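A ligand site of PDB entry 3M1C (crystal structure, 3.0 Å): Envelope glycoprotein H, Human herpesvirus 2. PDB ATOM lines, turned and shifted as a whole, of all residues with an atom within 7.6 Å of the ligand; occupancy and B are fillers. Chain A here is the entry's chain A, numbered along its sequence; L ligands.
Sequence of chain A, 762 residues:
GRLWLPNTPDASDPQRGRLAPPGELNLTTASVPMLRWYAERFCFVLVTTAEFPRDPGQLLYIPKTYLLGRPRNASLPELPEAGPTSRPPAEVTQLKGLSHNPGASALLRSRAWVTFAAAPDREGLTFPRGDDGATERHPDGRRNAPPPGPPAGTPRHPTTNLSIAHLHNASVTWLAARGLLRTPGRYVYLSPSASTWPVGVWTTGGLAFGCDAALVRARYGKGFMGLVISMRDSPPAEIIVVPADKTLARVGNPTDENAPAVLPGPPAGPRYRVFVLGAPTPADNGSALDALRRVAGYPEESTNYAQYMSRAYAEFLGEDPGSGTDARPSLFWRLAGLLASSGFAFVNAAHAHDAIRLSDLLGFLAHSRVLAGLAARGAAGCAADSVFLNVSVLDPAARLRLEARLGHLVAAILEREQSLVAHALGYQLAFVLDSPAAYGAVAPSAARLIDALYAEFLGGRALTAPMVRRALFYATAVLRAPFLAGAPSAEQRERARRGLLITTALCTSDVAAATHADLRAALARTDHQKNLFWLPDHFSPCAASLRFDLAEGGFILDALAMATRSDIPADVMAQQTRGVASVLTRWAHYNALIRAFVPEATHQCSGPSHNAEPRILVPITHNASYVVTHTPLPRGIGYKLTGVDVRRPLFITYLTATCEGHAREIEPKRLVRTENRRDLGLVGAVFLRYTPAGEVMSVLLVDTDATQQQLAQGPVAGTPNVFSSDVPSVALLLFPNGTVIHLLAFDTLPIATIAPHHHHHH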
ATOM      1  N   ILE A 594      -6.534  15.870   6.680  1.00  0.00           N
ATOM      2  CA  ILE A 594      -6.412  17.257   7.081  1.00  0.00           C
ATOM      3  C   ILE A 594      -7.121  17.500   8.401  1.00  0.00           C
ATOM      4  O   ILE A 594      -6.544  18.073   9.320  1.00  0.00           O
ATOM      5  CB  ILE A 594      -6.961  18.159   5.983  1.00  0.00           C
ATOM      6  CG1 ILE A 594      -6.143  17.926   4.718  1.00  0.00           C
ATOM      7  CG2 ILE A 594      -6.943  19.631   6.439  1.00  0.00           C
ATOM      8  CD1 ILE A 594      -6.187  19.068   3.731  1.00  0.00           C
ATOM      9  N   ARG A 595      -8.366  17.053   8.506  1.00  0.00           N
ATOM     10  CA  ARG A 595      -9.134  17.144   9.750  1.00  0.00           C
ATOM     11  C   ARG A 595      -8.351  16.627  10.944  1.00  0.00           C
ATOM     12  O   ARG A 595      -8.464  17.156  12.037  1.00  0.00           O
ATOM     13  CB  ARG A 595     -10.420  16.337   9.609  1.00  0.00           C
ATOM     14  CG  ARG A 595     -11.647  16.962  10.219  1.00  0.00           C
ATOM     15  CD  ARG A 595     -12.780  15.959  10.234  1.00  0.00           C
ATOM     16  NE  ARG A 595     -13.204  15.598   8.887  1.00  0.00           N
ATOM     17  CZ  ARG A 595     -13.637  14.387   8.554  1.00  0.00           C
ATOM     18  NH1 ARG A 595     -13.691  13.408   9.465  1.00  0.00           N
ATOM     19  NH2 ARG A 595     -14.007  14.143   7.292  1.00  0.00           N
ATOM     20  N   VAL A 598      -4.356  18.673  11.518  1.00  0.00           N
ATOM     21  CA  VAL A 598      -4.306  20.077  11.857  1.00  0.00           C
ATOM     22  C   VAL A 598      -4.891  20.254  13.243  1.00  0.00           C
ATOM     23  O   VAL A 598      -6.084  20.065  13.415  1.00  0.00           O
ATOM     24  CB  VAL A 598      -5.113  20.922  10.918  1.00  0.00           C
ATOM     25  CG1 VAL A 598      -5.150  22.343  11.429  1.00  0.00           C
ATOM     26  CG2 VAL A 598      -4.514  20.854   9.508  1.00  0.00           C
ATOM     27  N   PRO A 599      -4.050  20.587  14.224  1.00  0.00           N
ATOM     28  CA  PRO A 599      -4.483  20.779  15.616  1.00  0.00           C
ATOM     29  C   PRO A 599      -5.469  21.928  15.753  1.00  0.00           C
ATOM     30  O   PRO A 599      -5.130  23.047  15.374  1.00  0.00           O
ATOM     31  CB  PRO A 599      -3.190  21.134  16.338  1.00  0.00           C
ATOM     32  CG  PRO A 599      -2.120  20.534  15.524  1.00  0.00           C
ATOM     33  CD  PRO A 599      -2.583  20.645  14.099  1.00  0.00           C
ATOM     34  N   GLU A 600      -6.655  21.658  16.280  1.00  0.00           N
ATOM     35  CA  GLU A 600      -7.610  22.706  16.580  1.00  0.00           C
ATOM     36  C   GLU A 600      -7.651  22.928  18.093  1.00  0.00           C
ATOM     37  O   GLU A 600      -7.285  22.038  18.864  1.00  0.00           O
ATOM     38  CB  GLU A 600      -8.998  22.311  16.089  1.00  0.00           C
ATOM     39  CG  GLU A 600      -9.553  23.234  15.021  1.00  0.00           C
ATOM     40  CD  GLU A 600      -8.863  23.073  13.678  1.00  0.00           C
ATOM     41  OE1 GLU A 600      -8.680  21.924  13.211  1.00  0.00           O
ATOM     42  OE2 GLU A 600      -8.522  24.112  13.066  1.00  0.00           O
ATOM     43  N   CYS A 605     -12.048  30.318  19.390  1.00  0.00           N
ATOM     44  CA  CYS A 605     -11.085  31.403  19.378  1.00  0.00           C
ATOM     45  C   CYS A 605     -11.724  32.742  18.980  1.00  0.00           C
ATOM     46  O   CYS A 605     -12.387  32.835  17.943  1.00  0.00           O
ATOM     47  CB  CYS A 605      -9.916  31.053  18.436  1.00  0.00           C
ATOM     48  SG  CYS A 605      -8.544  30.062  19.218  1.00  0.00           S
ATOM     49  N   SER A 609     -12.170  33.758  12.141  1.00  0.00           N
ATOM     50  CA  SER A 609     -11.090  32.878  11.812  1.00  0.00           C
ATOM     51  C   SER A 609     -10.618  33.300  10.454  1.00  0.00           C
ATOM     52  O   SER A 609     -11.418  33.402   9.512  1.00  0.00           O
ATOM     53  CB  SER A 609     -11.611  31.449  11.748  1.00  0.00           C
ATOM     54  OG  SER A 609     -12.594  31.338  10.731  1.00  0.00           O
ATOM     55  N   HIS A 610      -9.336  33.531  10.311  1.00  0.00           N
ATOM     56  CA  HIS A 610      -8.785  33.772   9.002  1.00  0.00           C
ATOM     57  C   HIS A 610      -8.333  32.384   8.630  1.00  0.00           C
ATOM     58  O   HIS A 610      -7.203  31.996   8.889  1.00  0.00           O
ATOM     59  CB  HIS A 610      -7.621  34.738   9.048  1.00  0.00           C
ATOM     60  CG  HIS A 610      -8.035  36.177   8.963  1.00  0.00           C
ATOM     61  ND1 HIS A 610      -8.650  36.839   9.992  1.00  0.00           N
ATOM     62  CD2 HIS A 610      -7.923  37.078   7.952  1.00  0.00           C
ATOM     63  CE1 HIS A 610      -8.898  38.078   9.636  1.00  0.00           C
ATOM     64  NE2 HIS A 610      -8.464  38.245   8.404  1.00  0.00           N
ATOM     65  N   ASN A 611      -9.234  31.638   8.014  1.00  0.00           N
ATOM     66  CA  ASN A 611      -8.911  30.275   7.708  1.00  0.00           C
ATOM     67  C   ASN A 611      -8.311  30.258   6.342  1.00  0.00           C
ATOM     68  O   ASN A 611      -8.974  30.501   5.352  1.00  0.00           O
ATOM     69  CB  ASN A 611     -10.177  29.423   7.739  1.00  0.00           C
ATOM     70  CG  ASN A 611      -9.887  27.949   7.618  1.00  0.00           C
ATOM     71  OD1 ASN A 611      -9.334  27.486   6.619  1.00  0.00           O
ATOM     72  ND2 ASN A 611     -10.266  27.188   8.625  1.00  0.00           N
ATOM     73  N   ALA A 612      -7.013  29.977   6.300  1.00  0.00           N
ATOM     74  CA  ALA A 612      -6.341  29.836   5.025  1.00  0.00           C
ATOM     75  C   ALA A 612      -6.108  28.353   4.802  1.00  0.00           C
ATOM     76  O   ALA A 612      -5.630  27.653   5.697  1.00  0.00           O
ATOM     77  CB  ALA A 612      -5.034  30.587   5.034  1.00  0.00           C
ATOM     78  N   GLU A 613      -6.467  27.854   3.628  1.00  0.00           N
ATOM     79  CA  GLU A 613      -6.295  26.426   3.357  1.00  0.00           C
ATOM     80  C   GLU A 613      -4.831  26.096   3.092  1.00  0.00           C
ATOM     81  O   GLU A 613      -4.190  26.698   2.232  1.00  0.00           O
ATOM     82  CB  GLU A 613      -7.174  25.978   2.192  1.00  0.00           C
ATOM     83  CG  GLU A 613      -8.510  25.427   2.664  1.00  0.00           C
ATOM     84  CD  GLU A 613      -9.235  24.638   1.576  1.00  0.00           C
ATOM     85  OE1 GLU A 613      -8.683  24.517   0.464  1.00  0.00           O
ATOM     86  OE2 GLU A 613     -10.362  24.153   1.852  1.00  0.00           O
ATOM     87  N   PRO A 614      -4.308  25.144   3.866  1.00  0.00           N
ATOM     88  CA  PRO A 614      -2.903  24.780   3.854  1.00  0.00           C
ATOM     89  C   PRO A 614      -2.428  24.394   2.468  1.00  0.00           C
ATOM     90  O   PRO A 614      -3.042  23.554   1.821  1.00  0.00           O
ATOM     91  CB  PRO A 614      -2.836  23.561   4.783  1.00  0.00           C
ATOM     92  CG  PRO A 614      -4.206  23.110   4.954  1.00  0.00           C
ATOM     93  CD  PRO A 614      -5.059  24.334   4.821  1.00  0.00           C
ATOM     94  N   ARG A 615      -1.351  25.021   2.025  1.00  0.00           N
ATOM     95  CA  ARG A 615      -0.719  24.652   0.772  1.00  0.00           C
ATOM     96  C   ARG A 615       0.110  23.390   0.980  1.00  0.00           C
ATOM     97  O   ARG A 615       0.041  22.465   0.183  1.00  0.00           O
ATOM     98  CB  ARG A 615       0.183  25.789   0.283  1.00  0.00           C
ATOM     99  CG  ARG A 615      -0.488  27.080  -0.179  1.00  0.00           C
ATOM    100  CD  ARG A 615      -1.991  26.999  -0.359  1.00  0.00           C
ATOM    101  NE  ARG A 615      -2.392  26.008  -1.355  1.00  0.00           N
ATOM    102  CZ  ARG A 615      -3.655  25.769  -1.677  1.00  0.00           C
ATOM    103  NH1 ARG A 615      -4.626  26.439  -1.071  1.00  0.00           N
ATOM    104  NH2 ARG A 615      -3.948  24.845  -2.595  1.00  0.00           N
ATOM    105  N   LEU A 617       1.066  20.724   4.316  1.00  0.00           N
ATOM    106  CA  LEU A 617       0.821  20.357   5.713  1.00  0.00           C
ATOM    107  C   LEU A 617       1.865  19.358   6.206  1.00  0.00           C
ATOM    108  O   LEU A 617       1.985  18.256   5.680  1.00  0.00           O
ATOM    109  CB  LEU A 617      -0.579  19.766   5.881  1.00  0.00           C
ATOM    110  CG  LEU A 617      -0.958  19.143   7.228  1.00  0.00           C
ATOM    111  CD1 LEU A 617      -0.911  20.175   8.358  1.00  0.00           C
ATOM    112  CD2 LEU A 617      -2.337  18.510   7.160  1.00  0.00           C
ATOM    113  N   VAL A 627       2.175  24.439   8.881  1.00  0.00           N
ATOM    114  CA  VAL A 627       1.330  24.611   7.739  1.00  0.00           C
ATOM    115  C   VAL A 627       1.949  25.710   6.901  1.00  0.00           C
ATOM    116  O   VAL A 627       2.474  26.693   7.432  1.00  0.00           O
ATOM    117  CB  VAL A 627      -0.088  24.935   8.195  1.00  0.00           C
ATOM    118  CG1 VAL A 627      -0.539  26.271   7.677  1.00  0.00           C
ATOM    119  CG2 VAL A 627      -1.018  23.814   7.808  1.00  0.00           C
ATOM    120  N   THR A 629       1.284  28.438   4.044  1.00  0.00           N
ATOM    121  CA  THR A 629       0.224  29.176   3.390  1.00  0.00           C
ATOM    122  C   THR A 629       0.690  30.504   2.765  1.00  0.00           C
ATOM    123  O   THR A 629       1.849  30.891   2.893  1.00  0.00           O
ATOM    124  CB  THR A 629      -0.899  29.455   4.385  1.00  0.00           C
ATOM    125  OG1 THR A 629      -0.434  30.397   5.346  1.00  0.00           O
ATOM    126  CG2 THR A 629      -1.255  28.187   5.110  1.00  0.00           C
ATOM    127  N   THR A 631      -0.708  33.329   3.558  1.00  0.00           N
ATOM    128  CA  THR A 631      -1.202  34.350   4.459  1.00  0.00           C
ATOM    129  C   THR A 631      -0.947  33.936   5.882  1.00  0.00           C
ATOM    130  O   THR A 631      -1.063  32.757   6.223  1.00  0.00           O
ATOM    131  CB  THR A 631      -2.710  34.541   4.308  1.00  0.00           C
ATOM    132  OG1 THR A 631      -3.145  33.986   3.066  1.00  0.00           O
ATOM    133  CG2 THR A 631      -3.053  35.992   4.370  1.00  0.00           C
ATOM    134  N   PRO A 632      -0.595  34.897   6.737  1.00  0.00           N
ATOM    135  CA  PRO A 632      -0.494  34.639   8.171  1.00  0.00           C
ATOM    136  C   PRO A 632      -1.778  34.003   8.686  1.00  0.00           C
ATOM    137  O   PRO A 632      -2.860  34.340   8.200  1.00  0.00           O
ATOM    138  CB  PRO A 632      -0.356  36.044   8.755  1.00  0.00           C
ATOM    139  CG  PRO A 632      -0.884  36.957   7.654  1.00  0.00           C
ATOM    140  CD  PRO A 632      -0.426  36.320   6.421  1.00  0.00           C
ATOM    141  N   LEU A 633      -1.681  33.090   9.656  1.00  0.00           N
ATOM    142  CA  LEU A 633      -2.892  32.646  10.347  1.00  0.00           C
ATOM    143  C   LEU A 633      -3.026  33.474  11.602  1.00  0.00           C
ATOM    144  O   LEU A 633      -2.083  34.146  11.999  1.00  0.00           O
ATOM    145  CB  LEU A 633      -2.809  31.174  10.696  1.00  0.00           C
ATOM    146  CG  LEU A 633      -2.461  30.272   9.535  1.00  0.00           C
ATOM    147  CD1 LEU A 633      -2.653  28.853   9.948  1.00  0.00           C
ATOM    148  CD2 LEU A 633      -3.341  30.610   8.378  1.00  0.00           C
ATOM    149  N   PRO A 634      -4.185  33.401  12.260  1.00  0.00           N
ATOM    150  CA  PRO A 634      -4.402  34.245  13.438  1.00  0.00           C
ATOM    151  C   PRO A 634      -3.863  33.571  14.698  1.00  0.00           C
ATOM    152  O   PRO A 634      -3.695  34.256  15.726  1.00  0.00           O
ATOM    153  CB  PRO A 634      -5.919  34.358  13.521  1.00  0.00           C
ATOM    154  CG  PRO A 634      -6.468  33.515  12.350  1.00  0.00           C
ATOM    155  CD  PRO A 634      -5.369  32.588  11.962  1.00  0.00           C
ATOM    156  N   ARG A 635      -3.599  32.266  14.627  1.00  0.00           N
ATOM    157  CA  ARG A 635      -3.065  31.547  15.780  1.00  0.00           C
ATOM    158  C   ARG A 635      -1.855  30.750  15.357  1.00  0.00           C
ATOM    159  O   ARG A 635      -1.617  30.582  14.168  1.00  0.00           O
ATOM    160  CB  ARG A 635      -4.123  30.625  16.406  1.00  0.00           C
ATOM    161  CG  ARG A 635      -4.720  29.641  15.434  1.00  0.00           C
ATOM    162  CD  ARG A 635      -5.683  28.669  16.088  1.00  0.00           C
ATOM    163  NE  ARG A 635      -6.048  27.648  15.113  1.00  0.00           N
ATOM    164  CZ  ARG A 635      -5.613  26.390  15.117  1.00  0.00           C
ATOM    165  NH1 ARG A 635      -4.826  25.965  16.085  1.00  0.00           N
ATOM    166  NH2 ARG A 635      -5.993  25.561  14.165  1.00  0.00           N
ATOM    167  N   GLY A 636      -1.072  30.289  16.333  1.00  0.00           N
ATOM    168  CA  GLY A 636       0.125  29.491  16.095  1.00  0.00           C
ATOM    169  C   GLY A 636       1.397  30.314  15.960  1.00  0.00           C
ATOM    170  O   GLY A 636       1.339  31.482  15.608  1.00  0.00           O
ATOM    171  N   THR A 653       3.545  28.278   9.544  1.00  0.00           N
ATOM    172  CA  THR A 653       2.928  28.463  10.837  1.00  0.00           C
ATOM    173  C   THR A 653       2.942  27.143  11.620  1.00  0.00           C
ATOM    174  O   THR A 653       2.724  26.062  11.064  1.00  0.00           O
ATOM    175  CB  THR A 653       1.521  29.012  10.667  1.00  0.00           C
ATOM    176  OG1 THR A 653       1.607  30.357  10.197  1.00  0.00           O
ATOM    177  CG2 THR A 653       0.733  28.986  11.984  1.00  0.00           C
ATOM    178  N   LEU A 655       1.173  25.069  14.289  1.00  0.00           N
ATOM    179  CA  LEU A 655      -0.125  24.969  14.903  1.00  0.00           C
ATOM    180  C   LEU A 655      -0.127  23.942  16.006  1.00  0.00           C
ATOM    181  O   LEU A 655       0.480  22.880  15.892  1.00  0.00           O
ATOM    182  CB  LEU A 655      -1.158  24.613  13.852  1.00  0.00           C
ATOM    183  CG  LEU A 655      -1.509  25.711  12.864  1.00  0.00           C
ATOM    184  CD1 LEU A 655      -2.433  25.157  11.797  1.00  0.00           C
ATOM    185  CD2 LEU A 655      -2.170  26.870  13.582  1.00  0.00           C
ATOM    186  N   THR A 658      -4.224  25.678  20.392  1.00  0.00           N
ATOM    187  CA  THR A 658      -4.172  26.922  21.113  1.00  0.00           C
ATOM    188  C   THR A 658      -4.673  28.062  20.226  1.00  0.00           C
ATOM    189  O   THR A 658      -4.669  27.966  19.010  1.00  0.00           O
ATOM    190  CB  THR A 658      -2.752  27.186  21.640  1.00  0.00           C
ATOM    191  OG1 THR A 658      -2.800  28.076  22.757  1.00  0.00           O
ATOM    192  CG2 THR A 658      -1.868  27.772  20.561  1.00  0.00           C
HETATM  193  C1  LIG L   1      -5.526  26.004   8.129  1.00  0.00           C
HETATM  194  C2  LIG L   1      -6.404  25.383   9.229  1.00  0.00           C
HETATM  195  C3  LIG L   1      -7.597  26.234   9.743  1.00  0.00           C
HETATM  196  C4  LIG L   1      -7.304  27.599  10.447  1.00  0.00           C
HETATM  197  C5  LIG L   1      -6.432  27.482  11.693  1.00  0.00           C
HETATM  198  O1  LIG L   1      -4.894  27.208   8.523  1.00  0.00           O
HETATM  199  O2  LIG L   1      -6.910  24.146   8.716  1.00  0.00           O
HETATM  200  O3  LIG L   1      -8.413  25.450  10.626  1.00  0.00           O
HETATM  201  O4  LIG L   1      -6.755  28.565   9.540  1.00  0.00           O
HETATM  202  O5  LIG L   1      -6.265  28.805  12.221  1.00  0.00           O
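The guanidinium group of Arg 635 lies within salt-bridge range of the side-chain carboxylate of Glu 600, 3.1 Å away. O of Pro 599 lies within hydrogen-bond range of NH2 of Arg 635 (2.9 Å).
The side-chain carboxylate of Glu 600 sits at hydrogen-bond distance from an oxygen (O3) of the ligand (2.8 Å). The backbone carbonyl oxygen (O) of Ala 612 sits close to an oxygen (O1) of the ligand, 3.0 Å away. O3 of the ligand sits close to ND2 of Asn 611 (3.2 Å). The guanidinium group (NE) of Arg 635 is in hydrogen-bond range of an oxygen (O5) of the ligand.
Val 598 touches the ligand (CG1 to O2, 3.7 Å). His 610 touches the ligand (O to O4, 3.5 Å). Pro 614 touches the ligand. Leu 633 touches the ligand. Pro 634 touches the ligand. Hydrophobic or aromatic side chains within 4 Å of the ligand: Val 598, Pro 614, Leu 633 and Pro 634. Within 4 Å of the ligand: Val 598, Glu 600, His 610, Asn 611, Ala 612, Pro 614, Leu 633, Pro 634 and Arg 635.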
